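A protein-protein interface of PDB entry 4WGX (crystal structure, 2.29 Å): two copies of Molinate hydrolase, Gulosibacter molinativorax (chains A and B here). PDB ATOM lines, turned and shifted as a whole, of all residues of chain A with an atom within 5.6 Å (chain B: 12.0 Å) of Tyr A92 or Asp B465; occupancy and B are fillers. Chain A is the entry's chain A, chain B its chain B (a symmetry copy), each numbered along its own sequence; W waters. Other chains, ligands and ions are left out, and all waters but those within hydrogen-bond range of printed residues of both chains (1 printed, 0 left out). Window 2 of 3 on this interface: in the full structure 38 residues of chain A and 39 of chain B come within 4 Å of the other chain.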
ATOM      1  N   GLY A  89     -14.378 -13.390  27.101  1.00  0.00           N
ATOM      2  CA  GLY A  89     -13.924 -14.595  27.771  1.00  0.00           C
ATOM      3  C   GLY A  89     -12.417 -14.769  27.713  1.00  0.00           C
ATOM      4  O   GLY A  89     -11.845 -15.476  28.537  1.00  0.00           O
ATOM      5  N   ASN A  90     -11.775 -14.114  26.751  1.00  0.00           N
ATOM      6  CA  ASN A  90     -10.352 -14.301  26.497  1.00  0.00           C
ATOM      7  C   ASN A  90      -9.518 -13.025  26.311  1.00  0.00           C
ATOM      8  O   ASN A  90      -8.481 -13.065  25.675  1.00  0.00           O
ATOM      9  CB  ASN A  90     -10.179 -15.173  25.247  1.00  0.00           C
ATOM     10  CG  ASN A  90     -10.557 -16.609  25.487  1.00  0.00           C
ATOM     11  OD1 ASN A  90      -9.942 -17.293  26.296  1.00  0.00           O
ATOM     12  ND2 ASN A  90     -11.546 -17.084  24.758  1.00  0.00           N
ATOM     13  N   TYR A  91      -9.961 -11.892  26.839  1.00  0.00           N
ATOM     14  CA  TYR A  91      -9.259 -10.638  26.593  1.00  0.00           C
ATOM     15  C   TYR A  91      -7.778 -10.668  27.066  1.00  0.00           C
ATOM     16  O   TYR A  91      -6.889 -10.152  26.373  1.00  0.00           O
ATOM     17  CB  TYR A  91     -10.027  -9.479  27.249  1.00  0.00           C
ATOM     18  CG  TYR A  91     -11.423  -9.254  26.679  1.00  0.00           C
ATOM     19  CD1 TYR A  91     -11.633  -9.124  25.315  1.00  0.00           C
ATOM     20  CD2 TYR A  91     -12.527  -9.189  27.511  1.00  0.00           C
ATOM     21  CE1 TYR A  91     -12.901  -8.938  24.802  1.00  0.00           C
ATOM     22  CE2 TYR A  91     -13.787  -9.000  27.013  1.00  0.00           C
ATOM     23  CZ  TYR A  91     -13.972  -8.859  25.660  1.00  0.00           C
ATOM     24  OH  TYR A  91     -15.241  -8.672  25.174  1.00  0.00           O
ATOM     25  N   TYR A  92      -7.501 -11.317  28.194  1.00  0.00           N
ATOM     26  CA  TYR A  92      -6.125 -11.364  28.713  1.00  0.00           C
ATOM     27  C   TYR A  92      -5.204 -12.122  27.763  1.00  0.00           C
ATOM     28  O   TYR A  92      -4.027 -11.786  27.628  1.00  0.00           O
ATOM     29  CB  TYR A  92      -6.082 -11.965  30.130  1.00  0.00           C
ATOM     30  CG  TYR A  92      -6.445 -13.430  30.267  1.00  0.00           C
ATOM     31  CD1 TYR A  92      -7.766 -13.834  30.370  1.00  0.00           C
ATOM     32  CD2 TYR A  92      -5.465 -14.403  30.335  1.00  0.00           C
ATOM     33  CE1 TYR A  92      -8.100 -15.161  30.501  1.00  0.00           C
ATOM     34  CE2 TYR A  92      -5.792 -15.742  30.462  1.00  0.00           C
ATOM     35  CZ  TYR A  92      -7.107 -16.111  30.550  1.00  0.00           C
ATOM     36  OH  TYR A  92      -7.452 -17.433  30.682  1.00  0.00           O
ATOM     37  N   LYS A  93      -5.755 -13.105  27.065  1.00  0.00           N
ATOM     38  CA  LYS A  93      -5.004 -13.836  26.049  1.00  0.00           C
ATOM     39  C   LYS A  93      -4.781 -13.037  24.765  1.00  0.00           C
ATOM     40  O   LYS A  93      -3.756 -13.192  24.095  1.00  0.00           O
ATOM     41  CB  LYS A  93      -5.712 -15.147  25.721  1.00  0.00           C
ATOM     42  CG  LYS A  93      -6.029 -15.981  26.933  1.00  0.00           C
ATOM     43  CD  LYS A  93      -6.007 -17.456  26.609  1.00  0.00           C
ATOM     44  CE  LYS A  93      -6.451 -18.265  27.805  1.00  0.00           C
ATOM     45  NZ  LYS A  93      -6.794 -19.654  27.423  1.00  0.00           N
ATOM     46  N   VAL A  94      -5.751 -12.201  24.406  1.00  0.00           N
ATOM     47  CA  VAL A  94      -5.571 -11.264  23.303  1.00  0.00           C
ATOM     48  C   VAL A  94      -4.405 -10.341  23.639  1.00  0.00           C
ATOM     49  O   VAL A  94      -3.499 -10.104  22.830  1.00  0.00           O
ATOM     50  CB  VAL A  94      -6.848 -10.417  23.042  1.00  0.00           C
ATOM     51  CG1 VAL A  94      -6.606  -9.398  21.946  1.00  0.00           C
ATOM     52  CG2 VAL A  94      -8.039 -11.299  22.691  1.00  0.00           C
ATOM     53  N   ILE A  95      -4.444  -9.826  24.856  1.00  0.00           N
ATOM     54  CA  ILE A  95      -3.393  -8.948  25.335  1.00  0.00           C
ATOM     55  C   ILE A  95      -2.025  -9.664  25.365  1.00  0.00           C
ATOM     56  O   ILE A  95      -1.023  -9.113  24.899  1.00  0.00           O
ATOM     57  CB  ILE A  95      -3.765  -8.381  26.725  1.00  0.00           C
ATOM     58  CG1 ILE A  95      -4.959  -7.427  26.586  1.00  0.00           C
ATOM     59  CG2 ILE A  95      -2.605  -7.634  27.338  1.00  0.00           C
ATOM     60  CD1 ILE A  95      -5.552  -6.984  27.883  1.00  0.00           C
ATOM     61  N   GLU A  96      -1.975 -10.892  25.872  1.00  0.00           N
ATOM     62  CA  GLU A  96      -0.715 -11.645  25.840  1.00  0.00           C
ATOM     63  C   GLU A  96      -0.211 -11.908  24.422  1.00  0.00           C
ATOM     64  O   GLU A  96       0.982 -11.775  24.139  1.00  0.00           O
ATOM     65  CB  GLU A  96      -0.868 -12.964  26.589  1.00  0.00           C
ATOM     66  CG  GLU A  96      -0.850 -12.781  28.099  1.00  0.00           C
ATOM     67  CD  GLU A  96      -1.589 -13.880  28.828  1.00  0.00           C
ATOM     68  OE1 GLU A  96      -1.781 -14.978  28.252  1.00  0.00           O
ATOM     69  OE2 GLU A  96      -1.990 -13.636  29.978  1.00  0.00           O
ATOM     70  N   GLU A  97      -1.117 -12.275  23.527  1.00  0.00           N
ATOM     71  CA  GLU A  97      -0.756 -12.452  22.125  1.00  0.00           C
ATOM     72  C   GLU A  97      -0.152 -11.176  21.536  1.00  0.00           C
ATOM     73  O   GLU A  97       0.875 -11.219  20.839  1.00  0.00           O
ATOM     74  CB  GLU A  97      -1.981 -12.885  21.313  1.00  0.00           C
ATOM     75  CG  GLU A  97      -1.780 -12.934  19.803  1.00  0.00           C
ATOM     76  CD  GLU A  97      -3.074 -13.254  19.041  1.00  0.00           C
ATOM     77  OE1 GLU A  97      -4.155 -12.808  19.475  1.00  0.00           O
ATOM     78  OE2 GLU A  97      -3.006 -13.952  18.011  1.00  0.00           O
ATOM     79  N   PRO A 119      -8.370  -7.197  32.255  1.00  0.00           N
ATOM     80  CA  PRO A 119      -7.526  -8.110  31.480  1.00  0.00           C
ATOM     81  C   PRO A 119      -6.072  -7.657  31.326  1.00  0.00           C
ATOM     82  O   PRO A 119      -5.200  -8.512  31.167  1.00  0.00           O
ATOM     83  CB  PRO A 119      -8.228  -8.164  30.114  1.00  0.00           C
ATOM     84  CG  PRO A 119      -9.044  -6.945  30.035  1.00  0.00           C
ATOM     85  CD  PRO A 119      -9.459  -6.631  31.436  1.00  0.00           C
ATOM     86  N   ILE A 122      -4.469  -8.825  34.494  1.00  0.00           N
ATOM     87  CA  ILE A 122      -4.260 -10.265  34.405  1.00  0.00           C
ATOM     88  C   ILE A 122      -3.059 -10.591  33.511  1.00  0.00           C
ATOM     89  O   ILE A 122      -2.159 -11.326  33.929  1.00  0.00           O
ATOM     90  CB  ILE A 122      -5.519 -10.982  33.888  1.00  0.00           C
ATOM     91  CG1 ILE A 122      -6.637 -10.866  34.920  1.00  0.00           C
ATOM     92  CG2 ILE A 122      -5.250 -12.455  33.619  1.00  0.00           C
ATOM     93  CD1 ILE A 122      -8.008 -11.244  34.388  1.00  0.00           C
ATOM     94  N   ALA A 123      -3.027 -10.038  32.299  1.00  0.00           N
ATOM     95  CA  ALA A 123      -1.915 -10.315  31.391  1.00  0.00           C
ATOM     96  C   ALA A 123      -0.550  -9.813  31.893  1.00  0.00           C
ATOM     97  O   ALA A 123       0.453 -10.527  31.762  1.00  0.00           O
ATOM     98  CB  ALA A 123      -2.201  -9.737  30.024  1.00  0.00           C
ATOM     99  N   ARG A 126       0.475 -12.225  34.695  1.00  0.00           N
ATOM    100  CA  ARG A 126       0.908 -13.508  34.156  1.00  0.00           C
ATOM    101  C   ARG A 126       2.231 -13.438  33.400  1.00  0.00           C
ATOM    102  O   ARG A 126       3.008 -14.379  33.449  1.00  0.00           O
ATOM    103  CB  ARG A 126      -0.138 -14.105  33.227  1.00  0.00           C
ATOM    104  CG  ARG A 126      -1.337 -14.684  33.914  1.00  0.00           C
ATOM    105  CD  ARG A 126      -2.393 -15.107  32.887  1.00  0.00           C
ATOM    106  NE  ARG A 126      -2.449 -16.553  32.693  1.00  0.00           N
ATOM    107  CZ  ARG A 126      -2.207 -17.191  31.552  1.00  0.00           C
ATOM    108  NH1 ARG A 126      -1.881 -16.538  30.451  1.00  0.00           N
ATOM    109  NH2 ARG A 126      -2.305 -18.509  31.515  1.00  0.00           N
ATOM    110  N   ARG B 459     -22.117 -13.539  31.057  1.00  0.00           N
ATOM    111  CA  ARG B 459     -20.928 -13.804  30.278  1.00  0.00           C
ATOM    112  C   ARG B 459     -19.719 -13.236  31.000  1.00  0.00           C
ATOM    113  O   ARG B 459     -19.720 -12.091  31.440  1.00  0.00           O
ATOM    114  CB  ARG B 459     -21.078 -13.221  28.867  1.00  0.00           C
ATOM    115  CG  ARG B 459     -22.023 -14.035  27.994  1.00  0.00           C
ATOM    116  CD  ARG B 459     -22.447 -13.353  26.704  1.00  0.00           C
ATOM    117  NE  ARG B 459     -23.214 -14.278  25.883  1.00  0.00           N
ATOM    118  CZ  ARG B 459     -24.084 -13.924  24.942  1.00  0.00           C
ATOM    119  NH1 ARG B 459     -24.326 -12.650  24.683  1.00  0.00           N
ATOM    120  NH2 ARG B 459     -24.714 -14.856  24.258  1.00  0.00           N
ATOM    121  N   THR B 460     -18.698 -14.070  31.126  1.00  0.00           N
ATOM    122  CA  THR B 460     -17.500 -13.751  31.881  1.00  0.00           C
ATOM    123  C   THR B 460     -16.442 -13.161  30.964  1.00  0.00           C
ATOM    124  O   THR B 460     -16.123 -13.731  29.925  1.00  0.00           O
ATOM    125  CB  THR B 460     -16.964 -15.016  32.575  1.00  0.00           C
ATOM    126  OG1 THR B 460     -17.964 -15.512  33.467  1.00  0.00           O
ATOM    127  CG2 THR B 460     -15.696 -14.738  33.356  1.00  0.00           C
ATOM    128  N   ALA B 461     -15.901 -12.016  31.351  1.00  0.00           N
ATOM    129  CA  ALA B 461     -14.939 -11.304  30.515  1.00  0.00           C
ATOM    130  C   ALA B 461     -13.639 -12.065  30.344  1.00  0.00           C
ATOM    131  O   ALA B 461     -13.089 -12.123  29.244  1.00  0.00           O
ATOM    132  CB  ALA B 461     -14.652  -9.937  31.095  1.00  0.00           C
ATOM    133  N   ASN B 462     -13.138 -12.623  31.441  1.00  0.00           N
ATOM    134  CA  ASN B 462     -11.867 -13.324  31.421  1.00  0.00           C
ATOM    135  C   ASN B 462     -11.908 -14.642  32.180  1.00  0.00           C
ATOM    136  O   ASN B 462     -11.782 -14.699  33.402  1.00  0.00           O
ATOM    137  CB  ASN B 462     -10.771 -12.432  31.980  1.00  0.00           C
ATOM    138  CG  ASN B 462     -10.575 -11.192  31.164  1.00  0.00           C
ATOM    139  OD1 ASN B 462      -9.938 -11.218  30.114  1.00  0.00           O
ATOM    140  ND2 ASN B 462     -11.122 -10.092  31.638  1.00  0.00           N
ATOM    141  N   VAL B 463     -12.077 -15.707  31.418  1.00  0.00           N
ATOM    142  CA  VAL B 463     -12.210 -17.037  31.967  1.00  0.00           C
ATOM    143  C   VAL B 463     -10.826 -17.639  32.183  1.00  0.00           C
ATOM    144  O   VAL B 463     -10.081 -17.872  31.234  1.00  0.00           O
ATOM    145  CB  VAL B 463     -13.059 -17.922  31.037  1.00  0.00           C
ATOM    146  CG1 VAL B 463     -13.041 -19.377  31.481  1.00  0.00           C
ATOM    147  CG2 VAL B 463     -14.483 -17.394  30.986  1.00  0.00           C
ATOM    148  N   LEU B 464     -10.488 -17.867  33.445  1.00  0.00           N
ATOM    149  CA  LEU B 464      -9.182 -18.402  33.811  1.00  0.00           C
ATOM    150  C   LEU B 464      -9.143 -19.915  33.631  1.00  0.00           C
ATOM    151  O   LEU B 464     -10.105 -20.614  33.947  1.00  0.00           O
ATOM    152  CB  LEU B 464      -8.848 -18.026  35.253  1.00  0.00           C
ATOM    153  CG  LEU B 464      -8.999 -16.534  35.542  1.00  0.00           C
ATOM    154  CD1 LEU B 464      -8.889 -16.249  37.021  1.00  0.00           C
ATOM    155  CD2 LEU B 464      -7.957 -15.750  34.771  1.00  0.00           C
ATOM    156  N   ASP B 465      -8.024 -20.404  33.108  1.00  0.00           N
ATOM    157  CA  ASP B 465      -7.844 -21.825  32.835  1.00  0.00           C
ATOM    158  C   ASP B 465      -7.908 -22.649  34.119  1.00  0.00           C
ATOM    159  O   ASP B 465      -7.495 -22.188  35.185  1.00  0.00           O
ATOM    160  CB  ASP B 465      -6.508 -22.058  32.125  1.00  0.00           C
ATOM    161  CG  ASP B 465      -6.472 -21.447  30.736  1.00  0.00           C
ATOM    162  OD1 ASP B 465      -7.490 -21.536  30.016  1.00  0.00           O
ATOM    163  OD2 ASP B 465      -5.421 -20.875  30.366  1.00  0.00           O
HETATM  164  O   HOH W   1      -9.966 -18.489  28.601  1.00  0.00           O
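Among the printed residues, pairs that only touch across the chains: Gly A89 with Asn B462 (3.6 Å), Tyr A91 with Ala B461 (3.5 Å), Tyr A92 with Leu B464 (3.7 Å), Tyr A92 with Asp B465 (3.9 Å), Pro A119 with Asn B462 (3.5 Å) and Ile A122 with Asn B462 (3.9 Å).
Gly A89 touches just these residues of chain B: Thr B460 (3.2 Å), Ala B461 (2.8 Å), Asn B462 (3.6 Å) and Val B463 (2.9 Å). Of the printed residues of chain B, Tyr A91 touches Ala B461 and Asn B462. Of chain B, only Asn B462 (3.1 Å), Val B463 (2.7 Å), Leu B464 (3.7 Å) and Asp B465 (3.9 Å) come within 4 Å of Tyr A92. Of chain B, only Asp B465 comes within 4 Å of Lys A93. No residue of chain B comes within 4 Å of Val A94. No residue of chain B comes within 4 Å of Glu A96. Pro A119 touches just one residue of chain B: Asn B462 (3.5 Å). Of chain B, only Asn B462 comes within 4 Å of Ile A122. Of the printed residues of chain A, Thr B460 touches Gly A89 (3.2 Å). Printed residues of chain A within 4 Å of Ala B461: Gly A89 (2.8 Å), Asn A90 (3.5 Å) and Tyr A91 (3.5 Å). Of the printed residues of chain A, Asn B462 touches Gly A89, Tyr A91, Tyr A92, Pro A119 and Ile A122. Of the printed residues of chain A, Leu B464 touches Tyr A92 (3.7 Å). Of chain A, only Tyr A92 (3.9 Å) and Lys A93 (3.3 Å) come within 4 Å of Asp B465. The nearest residue of chain B that does not touch Tyr A92 is Ala B461 (5.7 Å). The nearest residue of chain A that does not touch Asp B465 is Arg A126 (4.1 Å). The nearest printed residue of chain A that does not touch Leu B464 is Ile A122 (4.4 Å).
No position is printed for both chains.
Water W1 lies within hydrogen-bond range of OD1 of Asn A90, O of Val B463 and OH of Tyr A92.
The backbone NH (N) of Gly A89 lies close to the backbone carbonyl oxygen (O) of Thr B460 (3.3 Å). N of Gly A89 is in hydrogen-bond range of O of Ala B461 (2.8 Å). The backbone carbonyl oxygen (O) of Gly A89 is in hydrogen-bond range of the backbone NH (N) of Val B463, at 2.9 Å. The backbone NH of Asn A90 sits at hydrogen-bond distance from the backbone carbonyl oxygen of Ala B461, at 3.5 Å. OD1 of Asn B462 lies within hydrogen-bond range of N of Tyr A91. N of Tyr A92 sits at hydrogen-bond distance from OD1 of Asn B462 (3.1 Å). The side-chain hydroxyl (OH) of Tyr A92 sits at hydrogen-bond distance from the backbone carbonyl oxygen (O) of Val B463 (2.7 Å). The side-chain carboxylate (OD1) of Asp B465 is in salt-bridge range of the side-chain amino group (NZ) of Lys A93, at 3.3 Å.
Of the 7 printed residues of chain B, 6 touch a printed residue of chain A. Of the 13 printed residues of chain A, 7 touch a printed residue of chain B. Printed residues of chain A that touch a printed residue of chain B: Gly A89, Asn A90, Tyr A91, Tyr A92, Lys A93, Pro A119 and Ile A122. Hydrophobic or aromatic side chains of chain A that line the printed part of chain B: Tyr A91, Tyr A92, Pro A119 and Ile A122. Among the printed residues, 14 pairs touch across the chains. Among the printed residues, Asp or Glu carboxylates within 4 Å of a Lys or Arg side-chain nitrogen of the other chain: Lys A93 with Asp B465 (3.3 Å).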
